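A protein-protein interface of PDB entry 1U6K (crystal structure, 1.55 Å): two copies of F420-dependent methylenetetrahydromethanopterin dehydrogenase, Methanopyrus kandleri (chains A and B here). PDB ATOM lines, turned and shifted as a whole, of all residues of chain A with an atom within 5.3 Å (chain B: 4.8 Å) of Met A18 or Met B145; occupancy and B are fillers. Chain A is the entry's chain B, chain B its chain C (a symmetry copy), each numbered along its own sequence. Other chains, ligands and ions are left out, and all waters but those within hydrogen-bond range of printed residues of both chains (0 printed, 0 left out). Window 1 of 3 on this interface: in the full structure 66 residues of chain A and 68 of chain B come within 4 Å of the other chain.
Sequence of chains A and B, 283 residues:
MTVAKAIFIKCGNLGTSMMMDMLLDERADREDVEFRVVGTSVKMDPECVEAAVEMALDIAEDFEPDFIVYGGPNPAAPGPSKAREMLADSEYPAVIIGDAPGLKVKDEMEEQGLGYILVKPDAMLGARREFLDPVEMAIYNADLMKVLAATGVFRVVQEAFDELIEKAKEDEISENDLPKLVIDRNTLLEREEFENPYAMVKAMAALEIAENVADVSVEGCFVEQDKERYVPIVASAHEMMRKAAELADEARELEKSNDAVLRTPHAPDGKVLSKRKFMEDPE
O of Met A18 sits at hydrogen-bond distance from NZ of Lys A10 (3.3 Å).
The side-chain amide nitrogen of Asn A13 lies close to the side-chain sulfur of Met A18, 3.7 Å away.
ND2 of Asn A13 sits close to ND2 of Asn A141.
ND2 of Asn A141 sits at hydrogen-bond distance from SD of Met A18 (3.7 Å).
SD of Met B18 lies within hydrogen-bond range of ND2 of Asn B141 (3.8 Å).
The backbone NH (N) of Phe B154 is in hydrogen-bond range of the backbone carbonyl oxygen (O) of Leu B148 (3.0 Å).
Met B22 touches Asn A13.
Met A18 touches Met B22 (CE to CE, 3.9 Å).
Met B145 touches Met A18 (CE to CE, 3.9 Å).
Asn B141 touches Met A19 (CB to CE, 3.8 Å).
CB of Ala B149 touches CB of Ala A138 (3.6 Å).
CB of Ala A138 touches CD1 of Phe B154, 3.7 Å away.
CB of Asn A141 touches SD of Met B145 (3.8 Å).
Ala A142 touches Ala B142 (CB to O, 3.4 Å).
Met A145 touches Met B18.
Asn B141 touches Met A145 (CB to SD, 3.9 Å).
SD of Met B145 sits at hydrogen-bond distance from N of Ala A142 (3.6 Å).
SD of Met A145 sits at hydrogen-bond distance from N of Ala B142, at 3.7 Å.
SD of Met B145 sits close to O of Ala A138, 3.5 Å away.
Of the printed residues of chain A, Met B145 touches Met A18 (3.9 Å), Ala A138 (3.5 Å), Asn A141 (3.8 Å) and Ala A142 (3.6 Å).
Of the printed residues of chain B, Ala A142 touches Ala B142, Met B145 and Lys B146.
Of the printed residues of chain B, Ala A138 touches Met B145, Ala B149 and Phe B154.
Of the printed residues of chain A, Met B22 touches Asn A13 (3.7 Å) and Met A18 (3.9 Å).
Of the printed residues of chain B, Asn A13 touches Met B22.
The nearest printed residue of chain A that does not touch Met B19 is Ala A138 (4.1 Å).
Met A18 touches Met B22, and with the chains exchanged Met A22 touches Met B18.
Asn A141 touches Met B145, and with the chains exchanged Met A145 touches Asn B141.
Ala B142 touches its own counterpart, Ala A142.
Ala A142 touches Met B145, and with the chains exchanged Met A145 touches Ala B142.
Of the 17 pairs that touch across the chains among the printed residues, 11 have their exchanged pair printed and touching as well.
Of the 14 printed residues of chain B, 9 touch a printed residue of chain A.
Printed residues of chain B that touch a printed residue of chain A: Met B18, Met B19, Met B22, Asn B141, Ala B142, Met B145, Lys B146, Ala B149 and Phe B154.
Hydrophobic or aromatic side chains of chain B that line the printed part of chain A: Met B18, Met B19, Met B22, Ala B142, Met B145, Ala B149 and Phe B154.
Of the 15 printed residues of chain A, 8 touch a printed residue of chain B.
Among the printed residues, no Asp or Glu carboxylate lies within 4 Å of a Lys or Arg side-chain nitrogen of the other chain.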
ATOM      1  N   LYS A  10      28.112  -1.863  13.730  1.00  0.00           N
ATOM      2  CA  LYS A  10      27.793  -1.183  12.467  1.00  0.00           C
ATOM      3  C   LYS A  10      28.955  -0.395  11.901  1.00  0.00           C
ATOM      4  O   LYS A  10      29.414   0.575  12.501  1.00  0.00           O
ATOM      5  CB  LYS A  10      26.600  -0.237  12.677  1.00  0.00           C
ATOM      6  CG  LYS A  10      25.358  -0.942  13.145  1.00  0.00           C
ATOM      7  CD  LYS A  10      24.217   0.015  13.498  1.00  0.00           C
ATOM      8  CE  LYS A  10      22.991  -0.779  13.920  1.00  0.00           C
ATOM      9  NZ  LYS A  10      21.730   0.049  13.989  1.00  0.00           N
ATOM     10  N   ASN A  13      27.382   1.770   5.880  1.00  0.00           N
ATOM     11  CA  ASN A  13      25.937   1.765   6.041  1.00  0.00           C
ATOM     12  C   ASN A  13      25.189   0.959   4.992  1.00  0.00           C
ATOM     13  O   ASN A  13      25.500   0.997   3.798  1.00  0.00           O
ATOM     14  CB  ASN A  13      25.416   3.198   6.065  1.00  0.00           C
ATOM     15  CG  ASN A  13      23.947   3.272   6.428  1.00  0.00           C
ATOM     16  OD1 ASN A  13      23.522   2.792   7.489  1.00  0.00           O
ATOM     17  ND2 ASN A  13      23.157   3.875   5.543  1.00  0.00           N
ATOM     18  N   LEU A  14      24.184   0.251   5.474  1.00  0.00           N
ATOM     19  CA  LEU A  14      23.316  -0.585   4.669  1.00  0.00           C
ATOM     20  C   LEU A  14      21.916  -0.260   5.196  1.00  0.00           C
ATOM     21  O   LEU A  14      21.751   0.033   6.379  1.00  0.00           O
ATOM     22  CB  LEU A  14      23.671  -2.047   4.951  1.00  0.00           C
ATOM     23  CG  LEU A  14      23.774  -3.104   3.869  1.00  0.00           C
ATOM     24  CD1 LEU A  14      24.497  -2.572   2.657  1.00  0.00           C
ATOM     25  CD2 LEU A  14      24.484  -4.310   4.456  1.00  0.00           C
ATOM     26  N   GLY A  15      20.895  -0.278   4.340  1.00  0.00           N
ATOM     27  CA  GLY A  15      19.584   0.008   4.869  1.00  0.00           C
ATOM     28  C   GLY A  15      19.217  -0.995   5.951  1.00  0.00           C
ATOM     29  O   GLY A  15      18.598  -0.652   6.960  1.00  0.00           O
ATOM     30  N   THR A  16      19.632  -2.242   5.753  1.00  0.00           N
ATOM     31  CA  THR A  16      19.289  -3.266   6.720  1.00  0.00           C
ATOM     32  C   THR A  16      20.034  -3.101   8.034  1.00  0.00           C
ATOM     33  O   THR A  16      19.491  -3.383   9.102  1.00  0.00           O
ATOM     34  CB  THR A  16      19.577  -4.654   6.175  1.00  0.00           C
ATOM     35  OG1 THR A  16      18.838  -4.841   4.967  1.00  0.00           O
ATOM     36  CG2 THR A  16      19.103  -5.712   7.174  1.00  0.00           C
ATOM     37  N   SER A  17      21.277  -2.652   7.954  1.00  0.00           N
ATOM     38  CA  SER A  17      22.064  -2.479   9.169  1.00  0.00           C
ATOM     39  C   SER A  17      21.563  -1.282   9.966  1.00  0.00           C
ATOM     40  O   SER A  17      21.690  -1.228  11.197  1.00  0.00           O
ATOM     41  CB  SER A  17      23.563  -2.374   8.828  1.00  0.00           C
ATOM     42  OG  SER A  17      23.921  -1.203   8.122  1.00  0.00           O
ATOM     43  N   MET A  18      20.996  -0.306   9.256  1.00  0.00           N
ATOM     44  CA  MET A  18      20.448   0.878   9.907  1.00  0.00           C
ATOM     45  C   MET A  18      19.342   0.469  10.864  1.00  0.00           C
ATOM     46  O   MET A  18      19.287   0.918  12.004  1.00  0.00           O
ATOM     47  CB  MET A  18      19.811   1.845   8.893  1.00  0.00           C
ATOM     48  CG  MET A  18      20.757   2.623   8.021  1.00  0.00           C
ATOM     49  SD  MET A  18      19.857   4.190   7.260  1.00  0.00           S
ATOM     50  CE  MET A  18      19.914   5.275   8.859  1.00  0.00           C
ATOM     51  N   MET A  19      18.465  -0.397  10.370  1.00  0.00           N
ATOM     52  CA  MET A  19      17.283  -0.840  11.095  1.00  0.00           C
ATOM     53  C   MET A  19      17.293  -2.167  11.852  1.00  0.00           C
ATOM     54  O   MET A  19      16.426  -2.391  12.689  1.00  0.00           O
ATOM     55  CB  MET A  19      16.104  -0.876  10.105  1.00  0.00           C
ATOM     56  CG  MET A  19      15.437   0.470   9.821  1.00  0.00           C
ATOM     57  SD  MET A  19      14.180   0.771  11.218  1.00  0.00           S
ATOM     58  CE  MET A  19      14.147   2.682  11.304  1.00  0.00           C
ATOM     59  N   MET A  20      18.257  -3.037  11.568  1.00  0.00           N
ATOM     60  CA  MET A  20      18.273  -4.365  12.182  1.00  0.00           C
ATOM     61  C   MET A  20      17.936  -4.501  13.663  1.00  0.00           C
ATOM     62  O   MET A  20      17.066  -5.291  14.014  1.00  0.00           O
ATOM     63  CB  MET A  20      19.583  -5.102  11.870  1.00  0.00           C
ATOM     64  CG  MET A  20      20.843  -4.383  12.247  1.00  0.00           C
ATOM     65  SD  MET A  20      22.418  -5.433  11.714  1.00  0.00           S
ATOM     66  CE  MET A  20      23.723  -4.179  12.256  1.00  0.00           C
ATOM     67  N   ASP A  21      18.581  -3.734  14.526  1.00  0.00           N
ATOM     68  CA  ASP A  21      18.303  -3.869  15.957  1.00  0.00           C
ATOM     69  C   ASP A  21      16.944  -3.331  16.382  1.00  0.00           C
ATOM     70  O   ASP A  21      16.273  -3.913  17.247  1.00  0.00           O
ATOM     71  CB  ASP A  21      19.419  -3.200  16.774  1.00  0.00           C
ATOM     72  CG  ASP A  21      19.638  -1.740  16.400  1.00  0.00           C
ATOM     73  OD1 ASP A  21      20.051  -1.478  15.246  1.00  0.00           O
ATOM     74  OD2 ASP A  21      19.397  -0.854  17.255  1.00  0.00           O
ATOM     75  N   MET A  22      16.513  -2.225  15.776  1.00  0.00           N
ATOM     76  CA  MET A  22      15.230  -1.650  16.150  1.00  0.00           C
ATOM     77  C   MET A  22      14.044  -2.485  15.709  1.00  0.00           C
ATOM     78  O   MET A  22      12.968  -2.379  16.285  1.00  0.00           O
ATOM     79  CB  MET A  22      15.090  -0.242  15.576  1.00  0.00           C
ATOM     80  CG  MET A  22      16.163   0.691  16.068  1.00  0.00           C
ATOM     81  SD  MET A  22      15.869   2.482  15.458  1.00  0.00           S
ATOM     82  CE  MET A  22      17.388   2.628  14.264  1.00  0.00           C
ATOM     83  N   ALA A 138      20.779  10.832   2.510  1.00  0.00           N
ATOM     84  CA  ALA A 138      19.626  10.608   3.386  1.00  0.00           C
ATOM     85  C   ALA A 138      18.380  10.333   2.540  1.00  0.00           C
ATOM     86  O   ALA A 138      17.597   9.470   2.884  1.00  0.00           O
ATOM     87  CB  ALA A 138      19.388  11.820   4.273  1.00  0.00           C
ATOM     88  N   ASN A 141      18.561   6.817   1.283  1.00  0.00           N
ATOM     89  CA  ASN A 141      18.289   5.878   2.356  1.00  0.00           C
ATOM     90  C   ASN A 141      16.815   5.854   2.751  1.00  0.00           C
ATOM     91  O   ASN A 141      16.285   4.811   3.136  1.00  0.00           O
ATOM     92  CB  ASN A 141      19.207   6.157   3.567  1.00  0.00           C
ATOM     93  CG  ASN A 141      20.559   5.489   3.395  1.00  0.00           C
ATOM     94  OD1 ASN A 141      21.552   6.121   3.028  1.00  0.00           O
ATOM     95  ND2 ASN A 141      20.580   4.187   3.613  1.00  0.00           N
ATOM     96  N   ALA A 142      16.134   6.998   2.654  1.00  0.00           N
ATOM     97  CA  ALA A 142      14.712   7.026   2.976  1.00  0.00           C
ATOM     98  C   ALA A 142      13.959   6.157   1.970  1.00  0.00           C
ATOM     99  O   ALA A 142      13.073   5.391   2.327  1.00  0.00           O
ATOM    100  CB  ALA A 142      14.198   8.486   2.932  1.00  0.00           C
ATOM    101  N   MET A 145      14.802   2.490   2.630  1.00  0.00           N
ATOM    102  CA  MET A 145      14.133   2.053   3.878  1.00  0.00           C
ATOM    103  C   MET A 145      12.650   1.745   3.635  1.00  0.00           C
ATOM    104  O   MET A 145      12.070   0.808   4.194  1.00  0.00           O
ATOM    105  CB  MET A 145      14.286   3.115   4.967  1.00  0.00           C
ATOM    106  CG  MET A 145      13.599   2.781   6.292  1.00  0.00           C
ATOM    107  SD  MET A 145      14.101   4.061   7.661  1.00  0.00           S
ATOM    108  CE  MET A 145      15.960   3.592   7.737  1.00  0.00           C
ATOM    109  N   MET B  18      19.333   9.100  13.933  1.00  0.00           N
ATOM    110  CA  MET B  18      19.631   7.999  13.015  1.00  0.00           C
ATOM    111  C   MET B  18      20.720   8.412  12.029  1.00  0.00           C
ATOM    112  O   MET B  18      21.631   7.650  11.715  1.00  0.00           O
ATOM    113  CB  MET B  18      18.400   7.610  12.171  1.00  0.00           C
ATOM    114  CG  MET B  18      17.318   6.796  12.863  1.00  0.00           C
ATOM    115  SD  MET B  18      16.047   6.028  11.563  1.00  0.00           S
ATOM    116  CE  MET B  18      16.876   4.307  11.317  1.00  0.00           C
ATOM    117  N   MET B  19      20.613   9.640  11.539  1.00  0.00           N
ATOM    118  CA  MET B  19      21.524  10.153  10.533  1.00  0.00           C
ATOM    119  C   MET B  19      22.661  11.084  10.933  1.00  0.00           C
ATOM    120  O   MET B  19      23.588  11.278  10.138  1.00  0.00           O
ATOM    121  CB  MET B  19      20.703  10.932   9.487  1.00  0.00           C
ATOM    122  CG  MET B  19      19.980  10.131   8.429  1.00  0.00           C
ATOM    123  SD  MET B  19      21.245   9.553   7.101  1.00  0.00           S
ATOM    124  CE  MET B  19      21.070   7.737   7.506  1.00  0.00           C
ATOM    125  N   MET B  22      26.334  10.170  10.101  1.00  0.00           N
ATOM    126  CA  MET B  22      26.525   9.913   8.682  1.00  0.00           C
ATOM    127  C   MET B  22      26.517  11.181   7.827  1.00  0.00           C
ATOM    128  O   MET B  22      27.178  11.241   6.786  1.00  0.00           O
ATOM    129  CB  MET B  22      25.455   8.938   8.194  1.00  0.00           C
ATOM    130  CG  MET B  22      25.551   7.590   8.864  1.00  0.00           C
ATOM    131  SD  MET B  22      24.088   6.479   8.337  1.00  0.00           S
ATOM    132  CE  MET B  22      23.628   5.740  10.070  1.00  0.00           C
ATOM    133  N   ASN B 141       9.666   6.010   9.743  1.00  0.00           N
ATOM    134  CA  ASN B 141      10.969   6.617   9.744  1.00  0.00           C
ATOM    135  C   ASN B 141      11.467   6.938   8.339  1.00  0.00           C
ATOM    136  O   ASN B 141      12.252   7.876   8.178  1.00  0.00           O
ATOM    137  CB  ASN B 141      11.965   5.708  10.493  1.00  0.00           C
ATOM    138  CG  ASN B 141      11.923   5.960  11.984  1.00  0.00           C
ATOM    139  OD1 ASN B 141      11.321   5.194  12.756  1.00  0.00           O
ATOM    140  ND2 ASN B 141      12.520   7.073  12.397  1.00  0.00           N
ATOM    141  N   ALA B 142      11.036   6.181   7.338  1.00  0.00           N
ATOM    142  CA  ALA B 142      11.484   6.459   5.978  1.00  0.00           C
ATOM    143  C   ALA B 142      10.848   7.773   5.554  1.00  0.00           C
ATOM    144  O   ALA B 142      11.531   8.622   4.961  1.00  0.00           O
ATOM    145  CB  ALA B 142      11.102   5.347   5.052  1.00  0.00           C
ATOM    146  N   ASP B 143       9.566   7.948   5.870  1.00  0.00           N
ATOM    147  CA  ASP B 143       8.904   9.221   5.524  1.00  0.00           C
ATOM    148  C   ASP B 143       9.507  10.398   6.271  1.00  0.00           C
ATOM    149  O   ASP B 143       9.745  11.472   5.698  1.00  0.00           O
ATOM    150  CB  ASP B 143       7.397   9.151   5.819  1.00  0.00           C
ATOM    151  CG  ASP B 143       6.651   8.255   4.837  1.00  0.00           C
ATOM    152  OD1 ASP B 143       7.094   8.132   3.647  1.00  0.00           O
ATOM    153  OD2 ASP B 143       5.596   7.659   5.239  1.00  0.00           O
ATOM    154  N   LEU B 144       9.789  10.230   7.559  1.00  0.00           N
ATOM    155  CA  LEU B 144      10.370  11.318   8.335  1.00  0.00           C
ATOM    156  C   LEU B 144      11.760  11.674   7.815  1.00  0.00           C
ATOM    157  O   LEU B 144      12.120  12.842   7.739  1.00  0.00           O
ATOM    158  CB  LEU B 144      10.463  10.908   9.819  1.00  0.00           C
ATOM    159  CG  LEU B 144      11.182  11.899  10.724  1.00  0.00           C
ATOM    160  CD1 LEU B 144      10.486  13.255  10.661  1.00  0.00           C
ATOM    161  CD2 LEU B 144      11.203  11.354  12.167  1.00  0.00           C
ATOM    162  N   MET B 145      12.537  10.664   7.420  1.00  0.00           N
ATOM    163  CA  MET B 145      13.892  10.899   6.928  1.00  0.00           C
ATOM    164  C   MET B 145      13.822  11.728   5.637  1.00  0.00           C
ATOM    165  O   MET B 145      14.616  12.663   5.426  1.00  0.00           O
ATOM    166  CB  MET B 145      14.596   9.553   6.653  1.00  0.00           C
ATOM    167  CG  MET B 145      15.997   9.746   6.109  1.00  0.00           C
ATOM    168  SD  MET B 145      16.953   8.013   6.030  1.00  0.00           S
ATOM    169  CE  MET B 145      16.924   7.581   7.944  1.00  0.00           C
ATOM    170  N   LYS B 146      12.840  11.376   4.799  1.00  0.00           N
ATOM    171  CA  LYS B 146      12.671  12.088   3.537  1.00  0.00           C
ATOM    172  C   LYS B 146      12.313  13.536   3.822  1.00  0.00           C
ATOM    173  O   LYS B 146      12.854  14.451   3.188  1.00  0.00           O
ATOM    174  CB  LYS B 146      11.587  11.412   2.672  1.00  0.00           C
ATOM    175  CG  LYS B 146      11.209  12.230   1.396  1.00  0.00           C
ATOM    176  CD  LYS B 146      12.376  12.459   0.525  1.00  0.00           C
ATOM    177  CE  LYS B 146      11.939  12.919  -0.861  1.00  0.00           C
ATOM    178  NZ  LYS B 146      11.186  11.846  -1.547  1.00  0.00           N
ATOM    179  N   VAL B 147      11.433  13.758   4.794  1.00  0.00           N
ATOM    180  CA  VAL B 147      11.060  15.122   5.150  1.00  0.00           C
ATOM    181  C   VAL B 147      12.292  15.893   5.663  1.00  0.00           C
ATOM    182  O   VAL B 147      12.594  16.972   5.183  1.00  0.00           O
ATOM    183  CB  VAL B 147       9.988  15.160   6.263  1.00  0.00           C
ATOM    184  CG1 VAL B 147       9.826  16.585   6.783  1.00  0.00           C
ATOM    185  CG2 VAL B 147       8.650  14.608   5.716  1.00  0.00           C
ATOM    186  N   LEU B 148      13.007  15.344   6.649  1.00  0.00           N
ATOM    187  CA  LEU B 148      14.152  16.083   7.197  1.00  0.00           C
ATOM    188  C   LEU B 148      15.276  16.318   6.182  1.00  0.00           C
ATOM    189  O   LEU B 148      16.013  17.347   6.233  1.00  0.00           O
ATOM    190  CB  LEU B 148      14.663  15.341   8.461  1.00  0.00           C
ATOM    191  CG  LEU B 148      13.601  15.155   9.557  1.00  0.00           C
ATOM    192  CD1 LEU B 148      14.238  14.319  10.701  1.00  0.00           C
ATOM    193  CD2 LEU B 148      13.110  16.452  10.109  1.00  0.00           C
ATOM    194  N   ALA B 149      15.401  15.412   5.219  1.00  0.00           N
ATOM    195  CA  ALA B 149      16.443  15.555   4.191  1.00  0.00           C
ATOM    196  C   ALA B 149      16.044  16.550   3.111  1.00  0.00           C
ATOM    197  O   ALA B 149      16.729  17.560   2.911  1.00  0.00           O
ATOM    198  CB  ALA B 149      16.762  14.218   3.536  1.00  0.00           C
ATOM    199  N   ALA B 150      14.922  16.276   2.447  1.00  0.00           N
ATOM    200  CA  ALA B 150      14.517  17.141   1.335  1.00  0.00           C
ATOM    201  C   ALA B 150      14.093  18.546   1.689  1.00  0.00           C
ATOM    202  O   ALA B 150      14.080  19.397   0.797  1.00  0.00           O
ATOM    203  CB  ALA B 150      13.453  16.461   0.483  1.00  0.00           C
ATOM    204  N   PHE B 154      18.418  18.504   7.537  1.00  0.00           N
ATOM    205  CA  PHE B 154      19.689  17.805   7.738  1.00  0.00           C
ATOM    206  C   PHE B 154      20.892  18.647   7.342  1.00  0.00           C
ATOM    207  O   PHE B 154      21.984  18.431   7.872  1.00  0.00           O
ATOM    208  CB  PHE B 154      19.713  16.483   6.980  1.00  0.00           C
ATOM    209  CG  PHE B 154      18.925  15.388   7.643  1.00  0.00           C
ATOM    210  CD1 PHE B 154      18.544  14.273   6.909  1.00  0.00           C
ATOM    211  CD2 PHE B 154      18.609  15.441   9.004  1.00  0.00           C
ATOM    212  CE1 PHE B 154      17.849  13.199   7.511  1.00  0.00           C
ATOM    213  CE2 PHE B 154      17.917  14.374   9.614  1.00  0.00           C
ATOM    214  CZ  PHE B 154      17.541  13.261   8.862  1.00  0.00           C
